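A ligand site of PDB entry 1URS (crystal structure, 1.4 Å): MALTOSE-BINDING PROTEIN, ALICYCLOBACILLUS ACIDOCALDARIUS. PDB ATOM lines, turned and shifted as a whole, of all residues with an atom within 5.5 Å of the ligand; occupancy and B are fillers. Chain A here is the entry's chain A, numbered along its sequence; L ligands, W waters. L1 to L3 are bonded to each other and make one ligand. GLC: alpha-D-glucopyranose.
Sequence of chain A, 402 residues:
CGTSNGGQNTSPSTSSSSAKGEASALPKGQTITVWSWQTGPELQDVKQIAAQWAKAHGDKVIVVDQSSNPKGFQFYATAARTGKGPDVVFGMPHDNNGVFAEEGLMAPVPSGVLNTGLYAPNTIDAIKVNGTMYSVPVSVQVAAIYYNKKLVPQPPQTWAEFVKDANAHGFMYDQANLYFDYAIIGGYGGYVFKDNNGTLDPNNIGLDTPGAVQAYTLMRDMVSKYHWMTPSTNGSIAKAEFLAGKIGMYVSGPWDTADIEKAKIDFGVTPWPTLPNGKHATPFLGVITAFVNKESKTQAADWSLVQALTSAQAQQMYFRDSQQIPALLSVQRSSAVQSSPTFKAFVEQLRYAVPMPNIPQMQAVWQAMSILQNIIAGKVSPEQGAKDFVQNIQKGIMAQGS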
ATOM      1  N   TRP A  37      15.847 -30.146  13.732  1.00  0.00           N
ATOM      2  CA  TRP A  37      15.100 -28.933  13.960  1.00  0.00           C
ATOM      3  C   TRP A  37      13.665 -29.279  14.351  1.00  0.00           C
ATOM      4  O   TRP A  37      12.807 -28.415  14.485  1.00  0.00           O
ATOM      5  CB  TRP A  37      15.135 -28.026  12.734  1.00  0.00           C
ATOM      6  CG  TRP A  37      16.164 -26.935  12.850  1.00  0.00           C
ATOM      7  CD1 TRP A  37      15.973 -25.675  13.322  1.00  0.00           C
ATOM      8  CD2 TRP A  37      17.553 -27.024  12.504  1.00  0.00           C
ATOM      9  NE1 TRP A  37      17.149 -24.961  13.282  1.00  0.00           N
ATOM     10  CE2 TRP A  37      18.134 -25.774  12.788  1.00  0.00           C
ATOM     11  CE3 TRP A  37      18.364 -28.045  11.984  1.00  0.00           C
ATOM     12  CZ2 TRP A  37      19.483 -25.503  12.561  1.00  0.00           C
ATOM     13  CZ3 TRP A  37      19.713 -27.774  11.757  1.00  0.00           C
ATOM     14  CH2 TRP A  37      20.262 -26.516  12.045  1.00  0.00           C
ATOM     15  N   GLN A  38      13.418 -30.583  14.520  1.00  0.00           N
ATOM     16  CA  GLN A  38      12.115 -31.052  14.975  1.00  0.00           C
ATOM     17  C   GLN A  38      12.355 -31.446  16.432  1.00  0.00           C
ATOM     18  O   GLN A  38      13.383 -32.030  16.759  1.00  0.00           O
ATOM     19  CB  GLN A  38      11.653 -32.263  14.155  1.00  0.00           C
ATOM     20  CG  GLN A  38      11.416 -31.955  12.675  1.00  0.00           C
ATOM     21  CD  GLN A  38      10.436 -30.818  12.457  1.00  0.00           C
ATOM     22  OE1 GLN A  38       9.263 -30.912  12.838  1.00  0.00           O
ATOM     23  NE2 GLN A  38      10.900 -29.744  11.829  1.00  0.00           N
ATOM     24  N   THR A  39      11.413 -31.098  17.299  1.00  0.00           N
ATOM     25  CA  THR A  39      11.561 -31.394  18.719  1.00  0.00           C
ATOM     26  C   THR A  39      10.383 -32.201  19.243  1.00  0.00           C
ATOM     27  O   THR A  39       9.622 -32.780  18.482  1.00  0.00           O
ATOM     28  CB  THR A  39      11.690 -30.073  19.519  1.00  0.00           C
ATOM     29  OG1 THR A  39      11.967 -30.365  20.894  1.00  0.00           O
ATOM     30  CG2 THR A  39      10.409 -29.259  19.410  1.00  0.00           C
ATOM     31  N   SER A  67      15.976 -26.918  17.405  1.00  0.00           N
ATOM     32  CA  SER A  67      14.696 -26.237  17.218  1.00  0.00           C
ATOM     33  C   SER A  67      14.567 -24.877  17.882  1.00  0.00           C
ATOM     34  O   SER A  67      13.802 -24.022  17.422  1.00  0.00           O
ATOM     35  CB  SER A  67      13.543 -27.132  17.687  1.00  0.00           C
ATOM     36  OG  SER A  67      13.560 -27.299  19.087  1.00  0.00           O
ATOM     37  N   PHE A  73      16.830 -21.706  11.282  1.00  0.00           N
ATOM     38  CA  PHE A  73      17.149 -22.777  10.345  1.00  0.00           C
ATOM     39  C   PHE A  73      18.463 -22.537   9.614  1.00  0.00           C
ATOM     40  O   PHE A  73      19.203 -23.479   9.317  1.00  0.00           O
ATOM     41  CB  PHE A  73      16.028 -22.928   9.300  1.00  0.00           C
ATOM     42  CG  PHE A  73      14.691 -23.284   9.908  1.00  0.00           C
ATOM     43  CD1 PHE A  73      13.625 -22.387   9.847  1.00  0.00           C
ATOM     44  CD2 PHE A  73      14.491 -24.510  10.537  1.00  0.00           C
ATOM     45  CE1 PHE A  73      12.386 -22.706  10.413  1.00  0.00           C
ATOM     46  CE2 PHE A  73      13.260 -24.834  11.105  1.00  0.00           C
ATOM     47  CZ  PHE A  73      12.208 -23.932  11.043  1.00  0.00           C
ATOM     48  N   GLY A  91      14.877 -32.697   9.739  1.00  0.00           N
ATOM     49  CA  GLY A  91      13.797 -31.760  10.027  1.00  0.00           C
ATOM     50  C   GLY A  91      13.943 -30.342   9.510  1.00  0.00           C
ATOM     51  O   GLY A  91      13.410 -29.407  10.112  1.00  0.00           O
ATOM     52  N   PRO A  93      13.117 -27.387   6.902  1.00  0.00           N
ATOM     53  CA  PRO A  93      12.123 -26.992   5.887  1.00  0.00           C
ATOM     54  C   PRO A  93      12.887 -26.760   4.589  1.00  0.00           C
ATOM     55  O   PRO A  93      13.936 -26.108   4.578  1.00  0.00           O
ATOM     56  CB  PRO A  93      11.532 -25.712   6.467  1.00  0.00           C
ATOM     57  CG  PRO A  93      11.574 -25.969   7.948  1.00  0.00           C
ATOM     58  CD  PRO A  93      12.957 -26.575   8.130  1.00  0.00           C
ATOM     59  N   ASP A  95      12.783 -24.805   1.947  1.00  0.00           N
ATOM     60  CA  ASP A  95      13.160 -23.517   1.383  1.00  0.00           C
ATOM     61  C   ASP A  95      14.601 -23.151   1.713  1.00  0.00           C
ATOM     62  O   ASP A  95      15.289 -22.514   0.922  1.00  0.00           O
ATOM     63  CB  ASP A  95      12.233 -22.413   1.884  1.00  0.00           C
ATOM     64  CG  ASP A  95      12.288 -22.236   3.384  1.00  0.00           C
ATOM     65  OD1 ASP A  95      11.910 -23.187   4.093  1.00  0.00           O
ATOM     66  OD2 ASP A  95      12.735 -21.163   3.845  1.00  0.00           O
ATOM     67  N   ASN A  96      15.056 -23.571   2.889  1.00  0.00           N
ATOM     68  CA  ASN A  96      16.406 -23.266   3.352  1.00  0.00           C
ATOM     69  C   ASN A  96      17.533 -23.901   2.580  1.00  0.00           C
ATOM     70  O   ASN A  96      18.638 -23.344   2.512  1.00  0.00           O
ATOM     71  CB  ASN A  96      16.542 -23.682   4.821  1.00  0.00           C
ATOM     72  CG  ASN A  96      15.669 -22.861   5.727  1.00  0.00           C
ATOM     73  OD1 ASN A  96      15.956 -21.693   6.001  1.00  0.00           O
ATOM     74  ND2 ASN A  96      14.586 -23.461   6.202  1.00  0.00           N
ATOM     75  N   GLN A 141       3.853 -30.351   4.846  1.00  0.00           N
ATOM     76  CA  GLN A 141       3.089 -29.481   5.727  1.00  0.00           C
ATOM     77  C   GLN A 141       2.340 -28.365   5.037  1.00  0.00           C
ATOM     78  O   GLN A 141       2.864 -27.724   4.127  1.00  0.00           O
ATOM     79  CB  GLN A 141       4.032 -28.818   6.745  1.00  0.00           C
ATOM     80  CG  GLN A 141       4.927 -29.768   7.524  1.00  0.00           C
ATOM     81  CD  GLN A 141       5.827 -29.046   8.508  1.00  0.00           C
ATOM     82  OE1 GLN A 141       6.132 -29.575   9.578  1.00  0.00           O
ATOM     83  NE2 GLN A 141       6.263 -27.833   8.157  1.00  0.00           N
ATOM     84  N   ASP A 174       0.205 -15.689  13.721  1.00  0.00           N
ATOM     85  CA  ASP A 174       1.474 -15.008  13.449  1.00  0.00           C
ATOM     86  C   ASP A 174       1.226 -14.121  12.227  1.00  0.00           C
ATOM     87  O   ASP A 174       1.781 -14.341  11.145  1.00  0.00           O
ATOM     88  CB  ASP A 174       2.556 -16.043  13.165  1.00  0.00           C
ATOM     89  CG  ASP A 174       3.950 -15.585  13.556  1.00  0.00           C
ATOM     90  OD1 ASP A 174       4.095 -14.446  14.054  1.00  0.00           O
ATOM     91  OD2 ASP A 174       4.898 -16.369  13.357  1.00  0.00           O
ATOM     92  N   ASN A 177       4.022 -12.714   9.866  1.00  0.00           N
ATOM     93  CA  ASN A 177       4.955 -13.740   9.383  1.00  0.00           C
ATOM     94  C   ASN A 177       4.467 -14.171   8.001  1.00  0.00           C
ATOM     95  O   ASN A 177       3.406 -14.788   7.880  1.00  0.00           O
ATOM     96  CB  ASN A 177       4.959 -14.940  10.333  1.00  0.00           C
ATOM     97  CG  ASN A 177       5.975 -16.002   9.933  1.00  0.00           C
ATOM     98  OD1 ASN A 177       6.458 -16.028   8.803  1.00  0.00           O
ATOM     99  ND2 ASN A 177       6.289 -16.892  10.871  1.00  0.00           N
ATOM    100  N   TYR A 179       5.245 -16.517   6.155  1.00  0.00           N
ATOM    101  CA  TYR A 179       4.965 -17.942   6.010  1.00  0.00           C
ATOM    102  C   TYR A 179       3.473 -18.241   6.182  1.00  0.00           C
ATOM    103  O   TYR A 179       2.918 -19.085   5.483  1.00  0.00           O
ATOM    104  CB  TYR A 179       5.746 -18.768   7.030  1.00  0.00           C
ATOM    105  CG  TYR A 179       5.410 -20.235   6.968  1.00  0.00           C
ATOM    106  CD1 TYR A 179       5.917 -21.045   5.942  1.00  0.00           C
ATOM    107  CD2 TYR A 179       4.556 -20.811   7.903  1.00  0.00           C
ATOM    108  CE1 TYR A 179       5.572 -22.394   5.855  1.00  0.00           C
ATOM    109  CE2 TYR A 179       4.197 -22.164   7.816  1.00  0.00           C
ATOM    110  CZ  TYR A 179       4.716 -22.941   6.797  1.00  0.00           C
ATOM    111  OH  TYR A 179       4.368 -24.277   6.736  1.00  0.00           O
ATOM    112  N   PHE A 180       2.845 -17.555   7.134  1.00  0.00           N
ATOM    113  CA  PHE A 180       1.435 -17.768   7.383  1.00  0.00           C
ATOM    114  C   PHE A 180       0.506 -16.825   6.628  1.00  0.00           C
ATOM    115  O   PHE A 180      -0.482 -17.281   6.073  1.00  0.00           O
ATOM    116  CB  PHE A 180       1.127 -17.641   8.884  1.00  0.00           C
ATOM    117  CG  PHE A 180       1.781 -18.711   9.720  1.00  0.00           C
ATOM    118  CD1 PHE A 180       1.294 -20.018   9.710  1.00  0.00           C
ATOM    119  CD2 PHE A 180       2.898 -18.412  10.478  1.00  0.00           C
ATOM    120  CE1 PHE A 180       1.919 -21.014  10.451  1.00  0.00           C
ATOM    121  CE2 PHE A 180       3.531 -19.408  11.231  1.00  0.00           C
ATOM    122  CZ  PHE A 180       3.041 -20.708  11.206  1.00  0.00           C
ATOM    123  N   TRP A 255       3.461 -29.135  14.338  1.00  0.00           N
ATOM    124  CA  TRP A 255       4.524 -28.865  15.296  1.00  0.00           C
ATOM    125  C   TRP A 255       3.933 -28.454  16.649  1.00  0.00           C
ATOM    126  O   TRP A 255       4.636 -28.444  17.668  1.00  0.00           O
ATOM    127  CB  TRP A 255       5.449 -27.751  14.773  1.00  0.00           C
ATOM    128  CG  TRP A 255       4.723 -26.533  14.259  1.00  0.00           C
ATOM    129  CD1 TRP A 255       4.243 -25.486  14.989  1.00  0.00           C
ATOM    130  CD2 TRP A 255       4.378 -26.263  12.888  1.00  0.00           C
ATOM    131  NE1 TRP A 255       3.622 -24.567  14.164  1.00  0.00           N
ATOM    132  CE2 TRP A 255       3.688 -25.019  12.870  1.00  0.00           C
ATOM    133  CE3 TRP A 255       4.579 -26.938  11.685  1.00  0.00           C
ATOM    134  CZ2 TRP A 255       3.205 -24.461  11.689  1.00  0.00           C
ATOM    135  CZ3 TRP A 255       4.091 -26.368  10.498  1.00  0.00           C
ATOM    136  CH2 TRP A 255       3.416 -25.138  10.522  1.00  0.00           C
ATOM    137  N   ILE A 288       9.469 -31.019   4.848  1.00  0.00           N
ATOM    138  CA  ILE A 288      10.498 -31.167   5.878  1.00  0.00           C
ATOM    139  C   ILE A 288      11.466 -32.180   5.302  1.00  0.00           C
ATOM    140  O   ILE A 288      11.058 -33.237   4.815  1.00  0.00           O
ATOM    141  CB  ILE A 288       9.898 -31.653   7.207  1.00  0.00           C
ATOM    142  CG1 ILE A 288       8.890 -30.619   7.724  1.00  0.00           C
ATOM    143  CG2 ILE A 288      11.005 -31.886   8.231  1.00  0.00           C
ATOM    144  CD1 ILE A 288       9.485 -29.216   7.921  1.00  0.00           C
ATOM    145  N   MET A 356       6.911 -23.563  -1.187  1.00  0.00           N
ATOM    146  CA  MET A 356       7.760 -22.436  -0.916  1.00  0.00           C
ATOM    147  C   MET A 356       8.960 -22.410  -1.832  1.00  0.00           C
ATOM    148  O   MET A 356       9.516 -23.439  -2.171  1.00  0.00           O
ATOM    149  CB  MET A 356       8.225 -22.464   0.514  1.00  0.00           C
ATOM    150  CG  MET A 356       7.066 -22.131   1.401  1.00  0.00           C
ATOM    151  SD  MET A 356       7.466 -20.870   2.448  1.00  0.00           S
ATOM    152  CE  MET A 356       8.401 -22.072   3.435  1.00  0.00           C
ATOM    153  N   GLN A 363      15.466 -16.245   1.143  1.00  0.00           N
ATOM    154  CA  GLN A 363      15.855 -15.812   2.480  1.00  0.00           C
ATOM    155  C   GLN A 363      15.804 -14.288   2.587  1.00  0.00           C
ATOM    156  O   GLN A 363      15.541 -13.746   3.659  1.00  0.00           O
ATOM    157  CB  GLN A 363      17.255 -16.324   2.842  1.00  0.00           C
ATOM    158  CG  GLN A 363      17.375 -17.840   2.816  1.00  0.00           C
ATOM    159  CD  GLN A 363      16.326 -18.544   3.683  1.00  0.00           C
ATOM    160  OE1 GLN A 363      15.638 -19.461   3.233  1.00  0.00           O
ATOM    161  NE2 GLN A 363      16.219 -18.111   4.938  1.00  0.00           N
ATOM    162  N   TRP A 366      12.230 -13.537   3.531  1.00  0.00           N
ATOM    163  CA  TRP A 366      11.918 -13.746   4.941  1.00  0.00           C
ATOM    164  C   TRP A 366      12.549 -12.602   5.744  1.00  0.00           C
ATOM    165  O   TRP A 366      11.968 -12.110   6.709  1.00  0.00           O
ATOM    166  CB  TRP A 366      12.520 -15.063   5.459  1.00  0.00           C
ATOM    167  CG  TRP A 366      12.062 -16.330   4.769  1.00  0.00           C
ATOM    168  CD1 TRP A 366      12.864 -17.355   4.340  1.00  0.00           C
ATOM    169  CD2 TRP A 366      10.712 -16.756   4.534  1.00  0.00           C
ATOM    170  NE1 TRP A 366      12.099 -18.388   3.862  1.00  0.00           N
ATOM    171  CE2 TRP A 366      10.776 -18.054   3.979  1.00  0.00           C
ATOM    172  CE3 TRP A 366       9.451 -16.175   4.759  1.00  0.00           C
ATOM    173  CZ2 TRP A 366       9.630 -18.773   3.631  1.00  0.00           C
ATOM    174  CZ3 TRP A 366       8.314 -16.897   4.414  1.00  0.00           C
ATOM    175  CH2 TRP A 366       8.418 -18.183   3.856  1.00  0.00           C
ATOM    176  N   MET A 369      10.303  -9.305   5.430  1.00  0.00           N
ATOM    177  CA  MET A 369       8.891  -9.345   5.815  1.00  0.00           C
ATOM    178  C   MET A 369       8.517  -8.559   7.069  1.00  0.00           C
ATOM    179  O   MET A 369       7.332  -8.440   7.386  1.00  0.00           O
ATOM    180  CB  MET A 369       8.427 -10.791   5.967  1.00  0.00           C
ATOM    181  CG  MET A 369       9.108 -11.537   7.094  1.00  0.00           C
ATOM    182  SD  MET A 369       8.517 -13.224   7.208  1.00  0.00           S
ATOM    183  CE  MET A 369       9.052 -13.668   8.853  1.00  0.00           C
HETATM  184  C1  GLC L   1       9.398 -26.028  15.511  1.00  0.00           C
HETATM  185  C2  GLC L   1       9.152 -26.933  14.324  1.00  0.00           C
HETATM  186  C3  GLC L   1       9.312 -26.150  13.037  1.00  0.00           C
HETATM  187  C4  GLC L   1       8.238 -25.024  13.063  1.00  0.00           C
HETATM  188  C5  GLC L   1       8.546 -24.074  14.291  1.00  0.00           C
HETATM  189  C6  GLC L   1       7.564 -22.923  14.492  1.00  0.00           C
HETATM  190  O1  GLC L   1      10.736 -25.539  15.511  1.00  0.00           O
HETATM  191  O2  GLC L   1      10.065 -28.019  14.431  1.00  0.00           O
HETATM  192  O3  GLC L   1       9.063 -27.051  11.938  1.00  0.00           O
HETATM  193  O4  GLC L   1       8.451 -24.296  11.888  1.00  0.00           O
HETATM  194  O5  GLC L   1       8.544 -24.880  15.481  1.00  0.00           O
HETATM  195  O6  GLC L   1       7.925 -22.171  15.678  1.00  0.00           O
HETATM  196  C1  GLC L   2       7.114 -24.143  11.050  1.00  0.00           C
HETATM  197  C2  GLC L   2       7.337 -24.673   9.620  1.00  0.00           C
HETATM  198  C3  GLC L   2       8.463 -23.848   8.958  1.00  0.00           C
HETATM  199  C4  GLC L   2       8.092 -22.386   8.952  1.00  0.00           C
HETATM  200  C5  GLC L   2       7.823 -21.873  10.398  1.00  0.00           C
HETATM  201  C6  GLC L   2       7.372 -20.401  10.368  1.00  0.00           C
HETATM  202  O2  GLC L   2       7.707 -26.050   9.673  1.00  0.00           O
HETATM  203  O3  GLC L   2       8.658 -24.298   7.586  1.00  0.00           O
HETATM  204  O4  GLC L   2       9.207 -21.647   8.388  1.00  0.00           O
HETATM  205  O5  GLC L   2       6.757 -22.696  10.975  1.00  0.00           O
HETATM  206  O6  GLC L   2       7.377 -19.753  11.638  1.00  0.00           O
HETATM  207  C1  GLC L   3       9.164 -20.961   7.175  1.00  0.00           C
HETATM  208  C2  GLC L   3      10.486 -21.315   6.427  1.00  0.00           C
HETATM  209  C3  GLC L   3      11.717 -20.778   7.257  1.00  0.00           C
HETATM  210  C4  GLC L   3      11.557 -19.249   7.429  1.00  0.00           C
HETATM  211  C5  GLC L   3      10.229 -18.949   8.159  1.00  0.00           C
HETATM  212  C6  GLC L   3       9.971 -17.462   8.331  1.00  0.00           C
HETATM  213  O2  GLC L   3      10.558 -22.711   6.248  1.00  0.00           O
HETATM  214  O3  GLC L   3      12.920 -21.093   6.579  1.00  0.00           O
HETATM  215  O4  GLC L   3      12.652 -18.713   8.190  1.00  0.00           O
HETATM  216  O5  GLC L   3       9.086 -19.518   7.399  1.00  0.00           O
HETATM  217  O6  GLC L   3       8.923 -17.280   9.270  1.00  0.00           O
HETATM  218  O   HOH W   1       9.604 -16.090  11.694  1.00  0.00           O
HETATM  219  O   HOH W   2      15.231 -19.376   7.350  1.00  0.00           O
HETATM  220  O   HOH W   3       7.298 -29.155  12.066  1.00  0.00           O
HETATM  221  O   HOH W   4       6.544 -25.749   6.308  1.00  0.00           O
HETATM  222  O   HOH W   5       8.971 -29.976  16.012  1.00  0.00           O
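Water W5 lies within hydrogen-bond range of an oxygen (O2) of GLC L1 (2.7 Å), the backbone NH (N) of Thr 39 (3.0 Å) and the side-chain amide oxygen (OE1) of Gln 38 (3.3 Å). Water W3 lies within hydrogen-bond range of OE1 of Gln 38, O3 of GLC L1 and OE1 of Gln 141. Water W2 lies within hydrogen-bond range of OD1 of Asn 96 (2.8 Å), O4 of GLC L3 (2.8 Å) and NE2 of Gln 363 (2.9 Å). Water W4 lies within hydrogen-bond range of the side-chain hydroxyl (OH) of Tyr 179 (2.7 Å), the side-chain amide nitrogen (NE2) of Gln 141 (2.8 Å) and an oxygen (O3) of GLC L2 (2.9 Å).
An oxygen (O2) of GLC L3 lies within hydrogen-bond range of the side-chain carboxylate (OD1) of Asp 95, at 2.6 Å. The side-chain amide nitrogen of Gln 141 sits at hydrogen-bond distance from an oxygen (O2) of GLC L2 (2.7 Å). O2 of GLC L1 is in hydrogen-bond range of O of Trp 37. The side-chain amide oxygen (OD1) of Asn 177 lies within hydrogen-bond range of an oxygen (O6) of GLC L3 (2.8 Å). An oxygen (O3) of GLC L3 is in hydrogen-bond range of the side-chain amide nitrogen (ND2) of Asn 96, at 2.9 Å. The side-chain amide nitrogen (NE2) of Gln 38 lies within hydrogen-bond range of an oxygen (O2) of GLC L1 (3.2 Å).
OD1 of Asp 95 lies within hydrogen-bond range of ND2 of Asn 96 (3.4 Å). OD2 of Asp 95 lies within hydrogen-bond range of NE1 of Trp 366, at 2.8 Å. OE1 of Gln 363 sits close to OD2 of Asp 95 (3.4 Å). The side-chain amide oxygen (OD1) of Asn 177 lies within hydrogen-bond range of the backbone NH (N) of Tyr 179 (3.0 Å). The side-chain amide nitrogen (ND2) of Asn 177 lies within hydrogen-bond range of the side-chain carboxylate (OD2) of Asp 174 (2.9 Å). O of Pro 93 is in hydrogen-bond range of ND2 of Asn 96, 3.2 Å away. O of Gly 91 lies within hydrogen-bond range of NE2 of Gln 38 (3.1 Å).
CB of Ser 67 touches O1 of GLC L1 (3.9 Å). CD1 of Phe 73 touches O3 of GLC L3 (3.6 Å). Pro 93 touches the ligand. CB of Tyr 179 touches O5 of GLC L3, 3.4 Å away. CE2 of Phe 180 touches O6 of GLC L2, at 3.9 Å. Trp 255 touches the ligand. Met 356 touches the ligand. NE1 of Trp 366 touches C4 of GLC L3 (3.7 Å). Met 369 touches the ligand. Hydrophobic or aromatic side chains within 4 Å of the ligand: Phe 73, Pro 93, Tyr 179, Phe 180, Trp 255, Met 356, Trp 366 and Met 369. Of the 20 residues printed, 15 come within 4 Å of the ligand.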
